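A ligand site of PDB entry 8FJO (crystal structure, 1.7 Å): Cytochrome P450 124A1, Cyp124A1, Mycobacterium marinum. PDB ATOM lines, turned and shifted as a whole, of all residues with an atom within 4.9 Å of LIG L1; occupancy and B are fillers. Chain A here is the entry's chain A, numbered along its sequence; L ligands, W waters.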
ATOM      1  N   SER A  86      27.147 -14.713 -13.987  1.00  0.00           N
ATOM      2  CA  SER A  86      26.197 -14.380 -15.025  1.00  0.00           C
ATOM      3  C   SER A  86      25.420 -15.601 -15.440  1.00  0.00           C
ATOM      4  O   SER A  86      24.297 -15.505 -15.912  1.00  0.00           O
ATOM      5  CB  SER A  86      26.927 -13.815 -16.216  1.00  0.00           C
ATOM      6  OG  SER A  86      27.647 -12.674 -15.790  1.00  0.00           O
ATOM      7  N   MET A 114      12.995  -5.461 -18.196  1.00  0.00           N
ATOM      8  CA  MET A 114      13.502  -6.849 -18.039  1.00  0.00           C
ATOM      9  C   MET A 114      14.826  -6.959 -17.295  1.00  0.00           C
ATOM     10  O   MET A 114      15.121  -8.072 -16.833  1.00  0.00           O
ATOM     11  CB  MET A 114      13.685  -7.499 -19.422  1.00  0.00           C
ATOM     12  CG  MET A 114      14.753  -6.815 -20.261  1.00  0.00           C
ATOM     13  SD  MET A 114      14.744  -7.378 -21.967  1.00  0.00           S
ATOM     14  CE  MET A 114      13.043  -7.023 -22.387  1.00  0.00           C
ATOM     15  N   ILE A 115      15.582  -5.869 -17.138  1.00  0.00           N
ATOM     16  CA  ILE A 115      16.891  -6.066 -16.582  1.00  0.00           C
ATOM     17  C   ILE A 115      16.808  -6.302 -15.082  1.00  0.00           C
ATOM     18  O   ILE A 115      17.779  -6.783 -14.502  1.00  0.00           O
ATOM     19  CB  ILE A 115      17.797  -4.870 -16.913  1.00  0.00           C
ATOM     20  CG1 ILE A 115      19.244  -5.336 -16.959  1.00  0.00           C
ATOM     21  CG2 ILE A 115      17.649  -3.702 -15.887  1.00  0.00           C
ATOM     22  CD1 ILE A 115      20.236  -4.279 -17.559  1.00  0.00           C
ATOM     23  N   HIS A 122      11.381 -12.758 -16.194  1.00  0.00           N
ATOM     24  CA  HIS A 122      12.364 -12.218 -17.131  1.00  0.00           C
ATOM     25  C   HIS A 122      12.227 -12.873 -18.496  1.00  0.00           C
ATOM     26  O   HIS A 122      12.104 -12.178 -19.513  1.00  0.00           O
ATOM     27  CB  HIS A 122      13.759 -12.377 -16.589  1.00  0.00           C
ATOM     28  CG  HIS A 122      14.818 -12.084 -17.601  1.00  0.00           C
ATOM     29  ND1 HIS A 122      15.520 -13.067 -18.246  1.00  0.00           N
ATOM     30  CD2 HIS A 122      15.231 -10.914 -18.144  1.00  0.00           C
ATOM     31  CE1 HIS A 122      16.387 -12.509 -19.082  1.00  0.00           C
ATOM     32  NE2 HIS A 122      16.235 -11.204 -19.032  1.00  0.00           N
ATOM     33  N   ARG A 126      11.433 -10.869 -21.938  1.00  0.00           N
ATOM     34  CA  ARG A 126      12.490 -10.836 -22.943  1.00  0.00           C
ATOM     35  C   ARG A 126      12.081 -11.585 -24.201  1.00  0.00           C
ATOM     36  O   ARG A 126      12.354 -11.122 -25.307  1.00  0.00           O
ATOM     37  CB  ARG A 126      13.768 -11.400 -22.394  1.00  0.00           C
ATOM     38  CG  ARG A 126      14.906 -11.217 -23.406  1.00  0.00           C
ATOM     39  CD  ARG A 126      16.244 -11.570 -22.771  1.00  0.00           C
ATOM     40  NE  ARG A 126      17.259 -11.733 -23.803  1.00  0.00           N
ATOM     41  CZ  ARG A 126      18.474 -11.198 -23.751  1.00  0.00           C
ATOM     42  NH1 ARG A 126      18.833 -10.453 -22.709  1.00  0.00           N
ATOM     43  NH2 ARG A 126      19.335 -11.416 -24.752  1.00  0.00           N
ATOM     44  N   PHE A 264       9.939  -0.653 -21.039  1.00  0.00           N
ATOM     45  CA  PHE A 264      11.023  -1.138 -21.920  1.00  0.00           C
ATOM     46  C   PHE A 264      11.653   0.043 -22.677  1.00  0.00           C
ATOM     47  O   PHE A 264      12.877   0.127 -22.811  1.00  0.00           O
ATOM     48  CB  PHE A 264      10.496  -2.206 -22.886  1.00  0.00           C
ATOM     49  CG  PHE A 264      11.534  -2.634 -23.898  1.00  0.00           C
ATOM     50  CD1 PHE A 264      12.654  -3.277 -23.476  1.00  0.00           C
ATOM     51  CD2 PHE A 264      11.404  -2.342 -25.252  1.00  0.00           C
ATOM     52  CE1 PHE A 264      13.630  -3.628 -24.357  1.00  0.00           C
ATOM     53  CE2 PHE A 264      12.397  -2.711 -26.150  1.00  0.00           C
ATOM     54  CZ  PHE A 264      13.501  -3.368 -25.704  1.00  0.00           C
ATOM     55  N   LEU A 267      13.889   1.811 -20.327  1.00  0.00           N
ATOM     56  CA  LEU A 267      15.165   1.087 -20.263  1.00  0.00           C
ATOM     57  C   LEU A 267      16.028   1.403 -21.462  1.00  0.00           C
ATOM     58  O   LEU A 267      17.228   1.650 -21.323  1.00  0.00           O
ATOM     59  CB  LEU A 267      14.886  -0.406 -20.138  1.00  0.00           C
ATOM     60  CG  LEU A 267      16.134  -1.307 -20.228  1.00  0.00           C
ATOM     61  CD1 LEU A 267      17.074  -1.024 -19.042  1.00  0.00           C
ATOM     62  CD2 LEU A 267      15.739  -2.788 -20.362  1.00  0.00           C
ATOM     63  N   LEU A 268      15.439   1.399 -22.653  1.00  0.00           N
ATOM     64  CA  LEU A 268      16.241   1.597 -23.851  1.00  0.00           C
ATOM     65  C   LEU A 268      16.880   2.975 -23.855  1.00  0.00           C
ATOM     66  O   LEU A 268      18.040   3.093 -24.228  1.00  0.00           O
ATOM     67  CB  LEU A 268      15.390   1.428 -25.116  1.00  0.00           C
ATOM     68  CG  LEU A 268      14.960   0.062 -25.620  1.00  0.00           C
ATOM     69  CD1 LEU A 268      14.304   0.212 -26.993  1.00  0.00           C
ATOM     70  CD2 LEU A 268      16.121  -0.887 -25.606  1.00  0.00           C
ATOM     71  N   ALA A 271      19.788   2.174 -21.147  1.00  0.00           N
ATOM     72  CA  ALA A 271      20.690   1.059 -21.414  1.00  0.00           C
ATOM     73  C   ALA A 271      21.128   0.972 -22.872  1.00  0.00           C
ATOM     74  O   ALA A 271      22.195   0.390 -23.141  1.00  0.00           O
ATOM     75  CB  ALA A 271      20.020  -0.240 -21.006  1.00  0.00           C
ATOM     76  N   GLY A 272      20.340   1.465 -23.822  1.00  0.00           N
ATOM     77  CA  GLY A 272      20.649   1.359 -25.239  1.00  0.00           C
ATOM     78  C   GLY A 272      21.383   2.609 -25.726  1.00  0.00           C
ATOM     79  O   GLY A 272      21.756   2.738 -26.899  1.00  0.00           O
ATOM     80  N   THR A 275      25.300   3.757 -22.961  1.00  0.00           N
ATOM     81  CA  THR A 275      26.299   2.724 -23.181  1.00  0.00           C
ATOM     82  C   THR A 275      26.990   2.907 -24.526  1.00  0.00           C
ATOM     83  O   THR A 275      28.213   3.036 -24.594  1.00  0.00           O
ATOM     84  CB  THR A 275      25.624   1.358 -23.125  1.00  0.00           C
ATOM     85  OG1 THR A 275      24.499   1.396 -23.993  1.00  0.00           O
ATOM     86  CG2 THR A 275      25.119   1.061 -21.722  1.00  0.00           C
ATOM     87  N   THR A 276      26.214   2.850 -25.599  1.00  0.00           N
ATOM     88  CA  THR A 276      26.768   3.020 -26.929  1.00  0.00           C
ATOM     89  C   THR A 276      27.491   4.356 -27.046  1.00  0.00           C
ATOM     90  O   THR A 276      28.570   4.427 -27.660  1.00  0.00           O
ATOM     91  CB  THR A 276      25.664   2.922 -27.963  1.00  0.00           C
ATOM     92  OG1 THR A 276      24.981   1.674 -27.796  1.00  0.00           O
ATOM     93  CG2 THR A 276      26.237   2.996 -29.371  1.00  0.00           C
ATOM     94  N   ALA A 279      30.813   3.872 -25.580  1.00  0.00           N
ATOM     95  CA  ALA A 279      31.674   3.051 -26.440  1.00  0.00           C
ATOM     96  C   ALA A 279      32.277   3.889 -27.557  1.00  0.00           C
ATOM     97  O   ALA A 279      33.433   3.695 -27.923  1.00  0.00           O
ATOM     98  CB  ALA A 279      30.893   1.887 -27.045  1.00  0.00           C
ATOM     99  N   VAL A 313      34.622  -2.319 -27.462  1.00  0.00           N
ATOM    100  CA  VAL A 313      33.771  -2.622 -26.324  1.00  0.00           C
ATOM    101  C   VAL A 313      34.589  -3.126 -25.171  1.00  0.00           C
ATOM    102  O   VAL A 313      34.365  -2.722 -24.034  1.00  0.00           O
ATOM    103  CB  VAL A 313      32.666  -3.602 -26.713  1.00  0.00           C
ATOM    104  CG1 VAL A 313      31.833  -3.843 -25.495  1.00  0.00           C
ATOM    105  CG2 VAL A 313      31.804  -2.939 -27.824  1.00  0.00           C
ATOM    106  N   PRO A 318      31.744   0.137 -21.325  1.00  0.00           N
ATOM    107  CA  PRO A 318      30.850   1.258 -20.960  1.00  0.00           C
ATOM    108  C   PRO A 318      30.050   1.004 -19.701  1.00  0.00           C
ATOM    109  O   PRO A 318      29.852   1.932 -18.901  1.00  0.00           O
ATOM    110  CB  PRO A 318      29.952   1.389 -22.205  1.00  0.00           C
ATOM    111  CG  PRO A 318      30.809   0.847 -23.316  1.00  0.00           C
ATOM    112  CD  PRO A 318      31.505  -0.321 -22.698  1.00  0.00           C
ATOM    113  N   VAL A 319      29.618  -0.239 -19.485  1.00  0.00           N
ATOM    114  CA  VAL A 319      29.054  -0.662 -18.221  1.00  0.00           C
ATOM    115  C   VAL A 319      30.168  -1.179 -17.336  1.00  0.00           C
ATOM    116  O   VAL A 319      30.734  -2.239 -17.572  1.00  0.00           O
ATOM    117  CB  VAL A 319      27.973  -1.730 -18.428  1.00  0.00           C
ATOM    118  CG1 VAL A 319      27.457  -2.142 -17.053  1.00  0.00           C
ATOM    119  CG2 VAL A 319      26.855  -1.097 -19.235  1.00  0.00           C
ATOM    120  N   MET A 322      27.636  -4.619 -13.048  1.00  0.00           N
ATOM    121  CA  MET A 322      26.214  -4.887 -12.722  1.00  0.00           C
ATOM    122  C   MET A 322      26.182  -5.593 -11.388  1.00  0.00           C
ATOM    123  O   MET A 322      27.108  -6.359 -11.063  1.00  0.00           O
ATOM    124  CB  MET A 322      25.611  -5.753 -13.808  1.00  0.00           C
ATOM    125  CG  MET A 322      25.322  -5.070 -15.175  1.00  0.00           C
ATOM    126  SD  MET A 322      23.765  -4.041 -14.943  1.00  0.00           S
ATOM    127  CE  MET A 322      23.694  -3.229 -16.500  1.00  0.00           C
ATOM    128  N   ARG A 324      24.204  -8.058  -8.508  1.00  0.00           N
ATOM    129  CA  ARG A 324      23.342  -9.214  -8.354  1.00  0.00           C
ATOM    130  C   ARG A 324      23.054  -9.290  -6.879  1.00  0.00           C
ATOM    131  O   ARG A 324      23.717  -8.651  -6.070  1.00  0.00           O
ATOM    132  CB  ARG A 324      24.074 -10.462  -8.858  1.00  0.00           C
ATOM    133  CG  ARG A 324      24.361 -10.526 -10.348  1.00  0.00           C
ATOM    134  CD  ARG A 324      23.094 -10.483 -11.097  1.00  0.00           C
ATOM    135  NE  ARG A 324      23.149 -10.798 -12.533  1.00  0.00           N
ATOM    136  CZ  ARG A 324      23.189  -9.886 -13.485  1.00  0.00           C
ATOM    137  NH1 ARG A 324      23.204  -8.577 -13.179  1.00  0.00           N
ATOM    138  NH2 ARG A 324      23.123 -10.260 -14.757  1.00  0.00           N
ATOM    139  N   TYR A 347      32.831  -5.669 -14.883  1.00  0.00           N
ATOM    140  CA  TYR A 347      33.231  -5.929 -16.255  1.00  0.00           C
ATOM    141  C   TYR A 347      34.503  -5.178 -16.595  1.00  0.00           C
ATOM    142  O   TYR A 347      35.282  -5.645 -17.434  1.00  0.00           O
ATOM    143  CB  TYR A 347      32.122  -5.517 -17.216  1.00  0.00           C
ATOM    144  CG  TYR A 347      30.774  -6.132 -16.892  1.00  0.00           C
ATOM    145  CD1 TYR A 347      30.613  -7.516 -16.750  1.00  0.00           C
ATOM    146  CD2 TYR A 347      29.665  -5.309 -16.705  1.00  0.00           C
ATOM    147  CE1 TYR A 347      29.360  -8.086 -16.434  1.00  0.00           C
ATOM    148  CE2 TYR A 347      28.441  -5.860 -16.393  1.00  0.00           C
ATOM    149  CZ  TYR A 347      28.299  -7.242 -16.308  1.00  0.00           C
ATOM    150  OH  TYR A 347      27.112  -7.777 -15.995  1.00  0.00           O
ATOM    151  N   GLY A 374      31.933  -6.933 -21.953  1.00  0.00           N
ATOM    152  CA  GLY A 374      31.342  -5.607 -21.820  1.00  0.00           C
ATOM    153  C   GLY A 374      29.845  -5.603 -21.984  1.00  0.00           C
ATOM    154  O   GLY A 374      29.158  -4.751 -21.403  1.00  0.00           O
ATOM    155  N   PHE A 375      29.311  -6.596 -22.707  1.00  0.00           N
ATOM    156  CA  PHE A 375      27.874  -6.793 -22.830  1.00  0.00           C
ATOM    157  C   PHE A 375      27.357  -7.729 -21.766  1.00  0.00           C
ATOM    158  O   PHE A 375      26.221  -8.195 -21.876  1.00  0.00           O
ATOM    159  CB  PHE A 375      27.523  -7.386 -24.199  1.00  0.00           C
ATOM    160  CG  PHE A 375      27.823  -6.472 -25.342  1.00  0.00           C
ATOM    161  CD1 PHE A 375      27.214  -5.235 -25.434  1.00  0.00           C
ATOM    162  CD2 PHE A 375      28.753  -6.846 -26.323  1.00  0.00           C
ATOM    163  CE1 PHE A 375      27.451  -4.403 -26.512  1.00  0.00           C
ATOM    164  CE2 PHE A 375      29.022  -5.967 -27.398  1.00  0.00           C
ATOM    165  CZ  PHE A 375      28.383  -4.758 -27.488  1.00  0.00           C
ATOM    166  N   GLY A 376      28.167  -8.027 -20.776  1.00  0.00           N
ATOM    167  CA  GLY A 376      27.831  -8.956 -19.725  1.00  0.00           C
ATOM    168  C   GLY A 376      28.608 -10.230 -19.884  1.00  0.00           C
ATOM    169  O   GLY A 376      29.189 -10.515 -20.927  1.00  0.00           O
ATOM    170  N   GLY A 377      28.613 -11.021 -18.813  1.00  0.00           N
ATOM    171  CA  GLY A 377      29.305 -12.301 -18.788  1.00  0.00           C
ATOM    172  C   GLY A 377      28.635 -13.413 -19.564  1.00  0.00           C
ATOM    173  O   GLY A 377      29.170 -14.527 -19.653  1.00  0.00           O
ATOM    174  N   GLY A 378      27.539 -13.169 -20.224  1.00  0.00           N
ATOM    175  CA  GLY A 378      26.831 -14.243 -20.886  1.00  0.00           C
ATOM    176  C   GLY A 378      25.555 -14.590 -20.122  1.00  0.00           C
ATOM    177  O   GLY A 378      25.315 -14.163 -18.989  1.00  0.00           O
ATOM    178  N   ALA A 380      21.533 -15.229 -19.187  1.00  0.00           N
ATOM    179  CA  ALA A 380      20.128 -14.874 -19.382  1.00  0.00           C
ATOM    180  C   ALA A 380      19.902 -13.406 -19.715  1.00  0.00           C
ATOM    181  O   ALA A 380      18.977 -13.082 -20.473  1.00  0.00           O
ATOM    182  CB  ALA A 380      19.355 -15.232 -18.129  1.00  0.00           C
ATOM    183  N   HIS A 381      20.678 -12.526 -19.133  1.00  0.00           N
ATOM    184  CA  HIS A 381      20.499 -11.091 -19.306  1.00  0.00           C
ATOM    185  C   HIS A 381      21.461 -10.510 -20.317  1.00  0.00           C
ATOM    186  O   HIS A 381      21.597  -9.284 -20.435  1.00  0.00           O
ATOM    187  CB  HIS A 381      20.644 -10.400 -17.964  1.00  0.00           C
ATOM    188  CG  HIS A 381      19.492 -10.653 -17.042  1.00  0.00           C
ATOM    189  ND1 HIS A 381      18.365  -9.857 -17.032  1.00  0.00           N
ATOM    190  CD2 HIS A 381      19.319 -11.584 -16.086  1.00  0.00           C
ATOM    191  CE1 HIS A 381      17.541 -10.290 -16.090  1.00  0.00           C
ATOM    192  NE2 HIS A 381      18.081 -11.357 -15.528  1.00  0.00           N
ATOM    193  N   PHE A 382      22.101 -11.370 -21.100  1.00  0.00           N
ATOM    194  CA  PHE A 382      23.079 -10.892 -22.076  1.00  0.00           C
ATOM    195  C   PHE A 382      22.503  -9.781 -22.928  1.00  0.00           C
ATOM    196  O   PHE A 382      21.392  -9.887 -23.421  1.00  0.00           O
ATOM    197  CB  PHE A 382      23.563 -12.004 -22.995  1.00  0.00           C
ATOM    198  CG  PHE A 382      24.605 -11.505 -23.954  1.00  0.00           C
ATOM    199  CD1 PHE A 382      25.899 -11.339 -23.522  1.00  0.00           C
ATOM    200  CD2 PHE A 382      24.245 -11.124 -25.245  1.00  0.00           C
ATOM    201  CE1 PHE A 382      26.888 -10.811 -24.366  1.00  0.00           C
ATOM    202  CE2 PHE A 382      25.221 -10.600 -26.108  1.00  0.00           C
ATOM    203  CZ  PHE A 382      26.516 -10.457 -25.668  1.00  0.00           C
ATOM    204  N   CYS A 383      23.235  -8.659 -22.977  1.00  0.00           N
ATOM    205  CA  CYS A 383      22.779  -7.445 -23.707  1.00  0.00           C
ATOM    206  C   CYS A 383      21.857  -7.774 -24.880  1.00  0.00           C
ATOM    207  O   CYS A 383      22.341  -8.349 -25.882  1.00  0.00           O
ATOM    208  CB  CYS A 383      23.979  -6.683 -24.236  1.00  0.00           C
ATOM    209  SG  CYS A 383      23.481  -5.203 -25.149  1.00  0.00           S
ATOM    210  N   LEU A 384      20.593  -7.358 -24.788  1.00  0.00           N
ATOM    211  CA  LEU A 384      19.676  -7.616 -25.875  1.00  0.00           C
ATOM    212  C   LEU A 384      20.082  -6.883 -27.122  1.00  0.00           C
ATOM    213  O   LEU A 384      19.762  -7.332 -28.247  1.00  0.00           O
ATOM    214  CB  LEU A 384      18.253  -7.185 -25.403  1.00  0.00           C
ATOM    215  CG  LEU A 384      17.173  -7.567 -26.384  1.00  0.00           C
ATOM    216  CD1 LEU A 384      17.027  -9.092 -26.307  1.00  0.00           C
ATOM    217  CD2 LEU A 384      15.907  -6.835 -25.976  1.00  0.00           C
ATOM    218  N   GLY A 385      20.740  -5.740 -26.974  1.00  0.00           N
ATOM    219  CA  GLY A 385      21.083  -4.995 -28.162  1.00  0.00           C
ATOM    220  C   GLY A 385      22.549  -5.150 -28.555  1.00  0.00           C
ATOM    221  O   GLY A 385      23.087  -4.286 -29.203  1.00  0.00           O
ATOM    222  N   LEU A 388      23.157  -4.688 -32.147  1.00  0.00           N
ATOM    223  CA  LEU A 388      22.841  -3.315 -32.525  1.00  0.00           C
ATOM    224  C   LEU A 388      23.989  -2.392 -32.088  1.00  0.00           C
ATOM    225  O   LEU A 388      24.412  -1.522 -32.845  1.00  0.00           O
ATOM    226  CB  LEU A 388      21.492  -2.885 -31.908  1.00  0.00           C
ATOM    227  CG  LEU A 388      21.149  -1.390 -32.138  1.00  0.00           C
ATOM    228  CD1 LEU A 388      21.167  -0.988 -33.619  1.00  0.00           C
ATOM    229  CD2 LEU A 388      19.781  -1.065 -31.552  1.00  0.00           C
ATOM    230  N   ALA A 389      24.486  -2.582 -30.869  1.00  0.00           N
ATOM    231  CA  ALA A 389      25.572  -1.689 -30.414  1.00  0.00           C
ATOM    232  C   ALA A 389      26.800  -1.851 -31.280  1.00  0.00           C
ATOM    233  O   ALA A 389      27.448  -0.860 -31.644  1.00  0.00           O
ATOM    234  CB  ALA A 389      25.938  -1.981 -28.940  1.00  0.00           C
ATOM    235  N   GLU A 392      26.166   0.052 -34.453  1.00  0.00           N
ATOM    236  CA  GLU A 392      26.291   1.492 -34.303  1.00  0.00           C
ATOM    237  C   GLU A 392      27.755   1.901 -34.252  1.00  0.00           C
ATOM    238  O   GLU A 392      28.165   2.877 -34.893  1.00  0.00           O
ATOM    239  CB  GLU A 392      25.573   1.970 -33.068  1.00  0.00           C
ATOM    240  CG  GLU A 392      24.054   1.650 -33.039  1.00  0.00           C
ATOM    241  CD  GLU A 392      23.327   2.380 -31.946  1.00  0.00           C
ATOM    242  OE1 GLU A 392      23.850   3.435 -31.554  1.00  0.00           O
ATOM    243  OE2 GLU A 392      22.193   1.942 -31.538  1.00  0.00           O
ATOM    244  N   ILE A 393      28.548   1.204 -33.443  1.00  0.00           N
ATOM    245  CA  ILE A 393      29.985   1.472 -33.399  1.00  0.00           C
ATOM    246  C   ILE A 393      30.624   1.356 -34.772  1.00  0.00           C
ATOM    247  O   ILE A 393      31.376   2.249 -35.201  1.00  0.00           O
ATOM    248  CB  ILE A 393      30.676   0.562 -32.397  1.00  0.00           C
ATOM    249  CG1 ILE A 393      30.103   0.851 -31.035  1.00  0.00           C
ATOM    250  CG2 ILE A 393      32.224   0.862 -32.355  1.00  0.00           C
ATOM    251  CD1 ILE A 393      30.362  -0.298 -30.030  1.00  0.00           C
HETATM  252  C1  LIG L   1      21.499  -5.445 -20.959  1.00  0.00           C
HETATM  253  C2  LIG L   1      25.894  -3.576 -21.913  1.00  0.00           C
HETATM  254  C3  LIG L   1      24.024  -1.366 -25.826  1.00  0.00           C
HETATM  255  C4  LIG L   1      19.595  -3.136 -24.720  1.00  0.00           C
HETATM  256  C5  LIG L   1      22.825  -5.147 -20.867  1.00  0.00           C
HETATM  257  C6  LIG L   1      23.774  -5.589 -19.851  1.00  0.00           C
HETATM  258  C7  LIG L   1      24.947  -5.050 -20.136  1.00  0.00           C
HETATM  259  C8  LIG L   1      24.835  -4.269 -21.338  1.00  0.00           C
HETATM  260  C9  LIG L   1      26.265  -5.208 -19.358  1.00  0.00           C
HETATM  261  C10 LIG L   1      23.590  -6.526 -18.612  1.00  0.00           C
HETATM  262  C11 LIG L   1      24.081  -7.904 -19.126  1.00  0.00           C
HETATM  263  C12 LIG L   1      23.979  -8.946 -18.000  1.00  0.00           C
HETATM  264  O1  LIG L   1      23.473  -8.624 -16.885  1.00  0.00           O
HETATM  265  O2  LIG L   1      24.433 -10.080 -18.185  1.00  0.00           O
HETATM  266  C13 LIG L   1      25.738  -2.777 -23.044  1.00  0.00           C
HETATM  267  C14 LIG L   1      26.765  -2.107 -23.723  1.00  0.00           C
HETATM  268  C15 LIG L   1      26.257  -1.494 -24.808  1.00  0.00           C
HETATM  269  C16 LIG L   1      24.856  -1.756 -24.806  1.00  0.00           C
HETATM  270  C17 LIG L   1      28.228  -2.114 -23.160  1.00  0.00           C
HETATM  271  C18 LIG L   1      26.877  -0.557 -25.872  1.00  0.00           C
HETATM  272  C19 LIG L   1      28.213  -0.553 -26.145  1.00  0.00           C
HETATM  273  C20 LIG L   1      22.687  -1.673 -25.878  1.00  0.00           C
HETATM  274  C21 LIG L   1      21.773  -1.305 -26.947  1.00  0.00           C
HETATM  275  C22 LIG L   1      20.549  -1.804 -26.637  1.00  0.00           C
HETATM  276  C23 LIG L   1      20.660  -2.487 -25.369  1.00  0.00           C
HETATM  277  C24 LIG L   1      22.121  -0.520 -28.217  1.00  0.00           C
HETATM  278  C25 LIG L   1      19.263  -1.610 -27.483  1.00  0.00           C
HETATM  279  C26 LIG L   1      18.340  -2.605 -27.587  1.00  0.00           C
HETATM  280  C27 LIG L   1      19.744  -3.866 -23.568  1.00  0.00           C
HETATM  281  C28 LIG L   1      18.716  -4.537 -22.843  1.00  0.00           C
HETATM  282  C29 LIG L   1      19.213  -5.172 -21.792  1.00  0.00           C
HETATM  283  C30 LIG L   1      20.669  -4.924 -21.882  1.00  0.00           C
HETATM  284  C31 LIG L   1      17.245  -4.455 -23.292  1.00  0.00           C
HETATM  285  C32 LIG L   1      18.594  -6.052 -20.705  1.00  0.00           C
HETATM  286  C33 LIG L   1      18.579  -7.500 -21.248  1.00  0.00           C
HETATM  287  C34 LIG L   1      17.998  -8.396 -20.154  1.00  0.00           C
HETATM  288  O3  LIG L   1      17.952  -7.991 -18.962  1.00  0.00           O
HETATM  289  O4  LIG L   1      17.632  -9.565 -20.433  1.00  0.00           O
HETATM  290  N1  LIG L   1      23.504  -4.311 -21.755  1.00  0.00           N
HETATM  291  N2  LIG L   1      24.588  -2.588 -23.757  1.00  0.00           N
HETATM  292  N3  LIG L   1      21.994  -2.467 -24.990  1.00  0.00           N
HETATM  293  N4  LIG L   1      20.940  -4.110 -22.945  1.00  0.00           N
HETATM  294 FE1  LIG L   1      22.793  -3.508 -23.452  1.00  0.00          FE
HETATM  295  C1  LG2 L   2      17.830   3.616 -11.436  1.00  0.00           C
HETATM  296  C2  LG2 L   2      17.453   4.239 -12.526  1.00  0.00           C
HETATM  297  C3  LG2 L   2      16.928   5.662 -12.523  1.00  0.00           C
HETATM  298  C4  LG2 L   2      18.622   6.631 -13.875  1.00  0.00           C
HETATM  299  C5  LG2 L   2      19.287   7.513 -12.832  1.00  0.00           C
HETATM  300  C6  LG2 L   2      22.825   1.389 -18.306  1.00  0.00           C
HETATM  301  C7  LG2 L   2      22.354  -0.057 -18.256  1.00  0.00           C
HETATM  302  C8  LG2 L   2      21.252  -0.398 -17.625  1.00  0.00           C
HETATM  303  C9  LG2 L   2      20.450   0.674 -16.927  1.00  0.00           C
HETATM  304  C10 LG2 L   2      19.356   0.196 -15.993  1.00  0.00           C
HETATM  305  C11 LG2 L   2      19.185   1.305 -14.969  1.00  0.00           C
HETATM  306  C12 LG2 L   2      19.538   1.162 -13.718  1.00  0.00           C
HETATM  307  C13 LG2 L   2      19.381   2.351 -12.775  1.00  0.00           C
HETATM  308  C14 LG2 L   2      18.388   2.214 -11.625  1.00  0.00           C
HETATM  309  C15 LG2 L   2      17.751   4.272 -10.074  1.00  0.00           C
HETATM  310  C16 LG2 L   2      18.610   2.628 -15.466  1.00  0.00           C
HETATM  311  C17 LG2 L   2      23.184  -1.082 -18.988  1.00  0.00           C
HETATM  312  O1  LG2 L   2      17.285   6.219 -13.750  1.00  0.00           O
HETATM  313  O2  LG2 L   2      19.253   6.287 -14.819  1.00  0.00           O
HETATM  314  O   HOH W   1      25.642 -10.919 -20.412  1.00  0.00           O
HETATM  315  O   HOH W   2      22.334  -1.685 -21.812  1.00  0.00           O
HETATM  316  O   HOH W   3      22.369  -6.849 -15.395  1.00  0.00           O
HETATM  317  O   HOH W   4      23.437 -12.565 -17.873  1.00  0.00           O
HETATM  318  O   HOH W   5      26.802 -10.381 -16.683  1.00  0.00           O
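N of Cys 383 sits at hydrogen-bond distance from O of Phe 375. The backbone carbonyl oxygen (O) of Ala 380 is in hydrogen-bond range of the guanidinium group (NH1) of Arg 126 (3.5 Å). ND1 of His 381 lies within hydrogen-bond range of NE2 of His 122. The side-chain sulfur (SG) of Cys 383 sits close to the backbone NH (N) of Gly 385 (3.3 Å). The side-chain hydroxyl (OG1) of Thr 275 lies within hydrogen-bond range of the backbone carbonyl oxygen (O) of Ala 271, at 2.7 Å. O of Phe 382 is in hydrogen-bond range of NH1 of Arg 126 (2.7 Å).
The guanidinium group (NH1) of Arg 126 lies within salt-bridge range of an oxygen (O4) of LIG L1 (2.7 Å). An oxygen (O4) of LIG L1 sits at hydrogen-bond distance from a ring nitrogen (NE2) of His 122 (2.6 Å). O3 of LIG L1 sits at hydrogen-bond distance from ND1 of His 381, at 2.7 Å. An oxygen (O1) of LIG L1 lies within salt-bridge range of the guanidinium group (NH2) of Arg 324 (2.7 Å). The side-chain sulfur of Cys 383 is bound to an iron atom (FE1) of LIG L1, 2.5 Å away.
The backbone carbonyl oxygen (O) of Ala 271 lies close to a nitrogen (N3) of LIG L1 (3.4 Å). Residues that only touch LIG L1: Met 114 (3.5 Å), Ile 115 (3.2 Å), Phe 264 (3.9 Å), Leu 267 (3.7 Å), Leu 268 (3.4 Å), Gly 272 (3.4 Å), Thr 275 (3.3 Å), Thr 276 (3.5 Å), Ala 279 (3.7 Å), Pro 318 (3.8 Å), Val 319 (3.8 Å), Met 322 (3.9 Å), Tyr 347 (3.7 Å), Gly 374 (3.3 Å), Phe 375 (3.5 Å), Gly 376 (3.7 Å), Ala 380 (3.8 Å), Phe 382 (3.9 Å), Leu 384 (3.6 Å), Gly 385 (3.6 Å) and Ala 389 (3.5 Å). Hydrophobic or aromatic side chains that line LIG L1: Met 114, Ile 115, His 122, Phe 264, Leu 267, Leu 268, Ala 279, Pro 318, Val 319, Met 322, Tyr 347, Phe 375, His 381, Leu 384 and Ala 389. Within 4 Å of LIG L1: Met 114, Ile 115, His 122, Arg 126, Phe 264, Leu 267, Leu 268, Ala 271, Gly 272, Thr 275, Thr 276, Ala 279, Pro 318, Val 319, Met 322, Arg 324, Tyr 347, Gly 374, Phe 375, Gly 376, Ala 380, His 381, Phe 382, Cys 383, Leu 384, Gly 385 and Ala 389.
Water W3 lies within hydrogen-bond range of an oxygen (O1) of LIG L1 (2.6 Å), the guanidinium group (NH1) of Arg 324 (2.9 Å) and the side-chain sulfur (SD) of Met 322 (3.2 Å). Water W1 lies within hydrogen-bond range of an oxygen (O2) of LIG L1 (2.7 Å), the backbone NH of Gly 378 (2.9 Å), the backbone carbonyl oxygen of Phe 375 (3.1 Å) and the backbone NH of Gly 377 (3.4 Å). Water W4 lies within hydrogen-bond range of O2 of LIG L1 (2.7 Å), O of Gly 378 (2.7 Å) and N of His 381 (3.0 Å). Water W5 lies within hydrogen-bond range of the side-chain hydroxyl (OG) of Ser 86 (2.6 Å), the side-chain hydroxyl (OH) of Tyr 347 (2.7 Å), an oxygen (O2) of LIG L1 (2.8 Å) and the backbone NH (N) of Gly 377 (2.9 Å).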
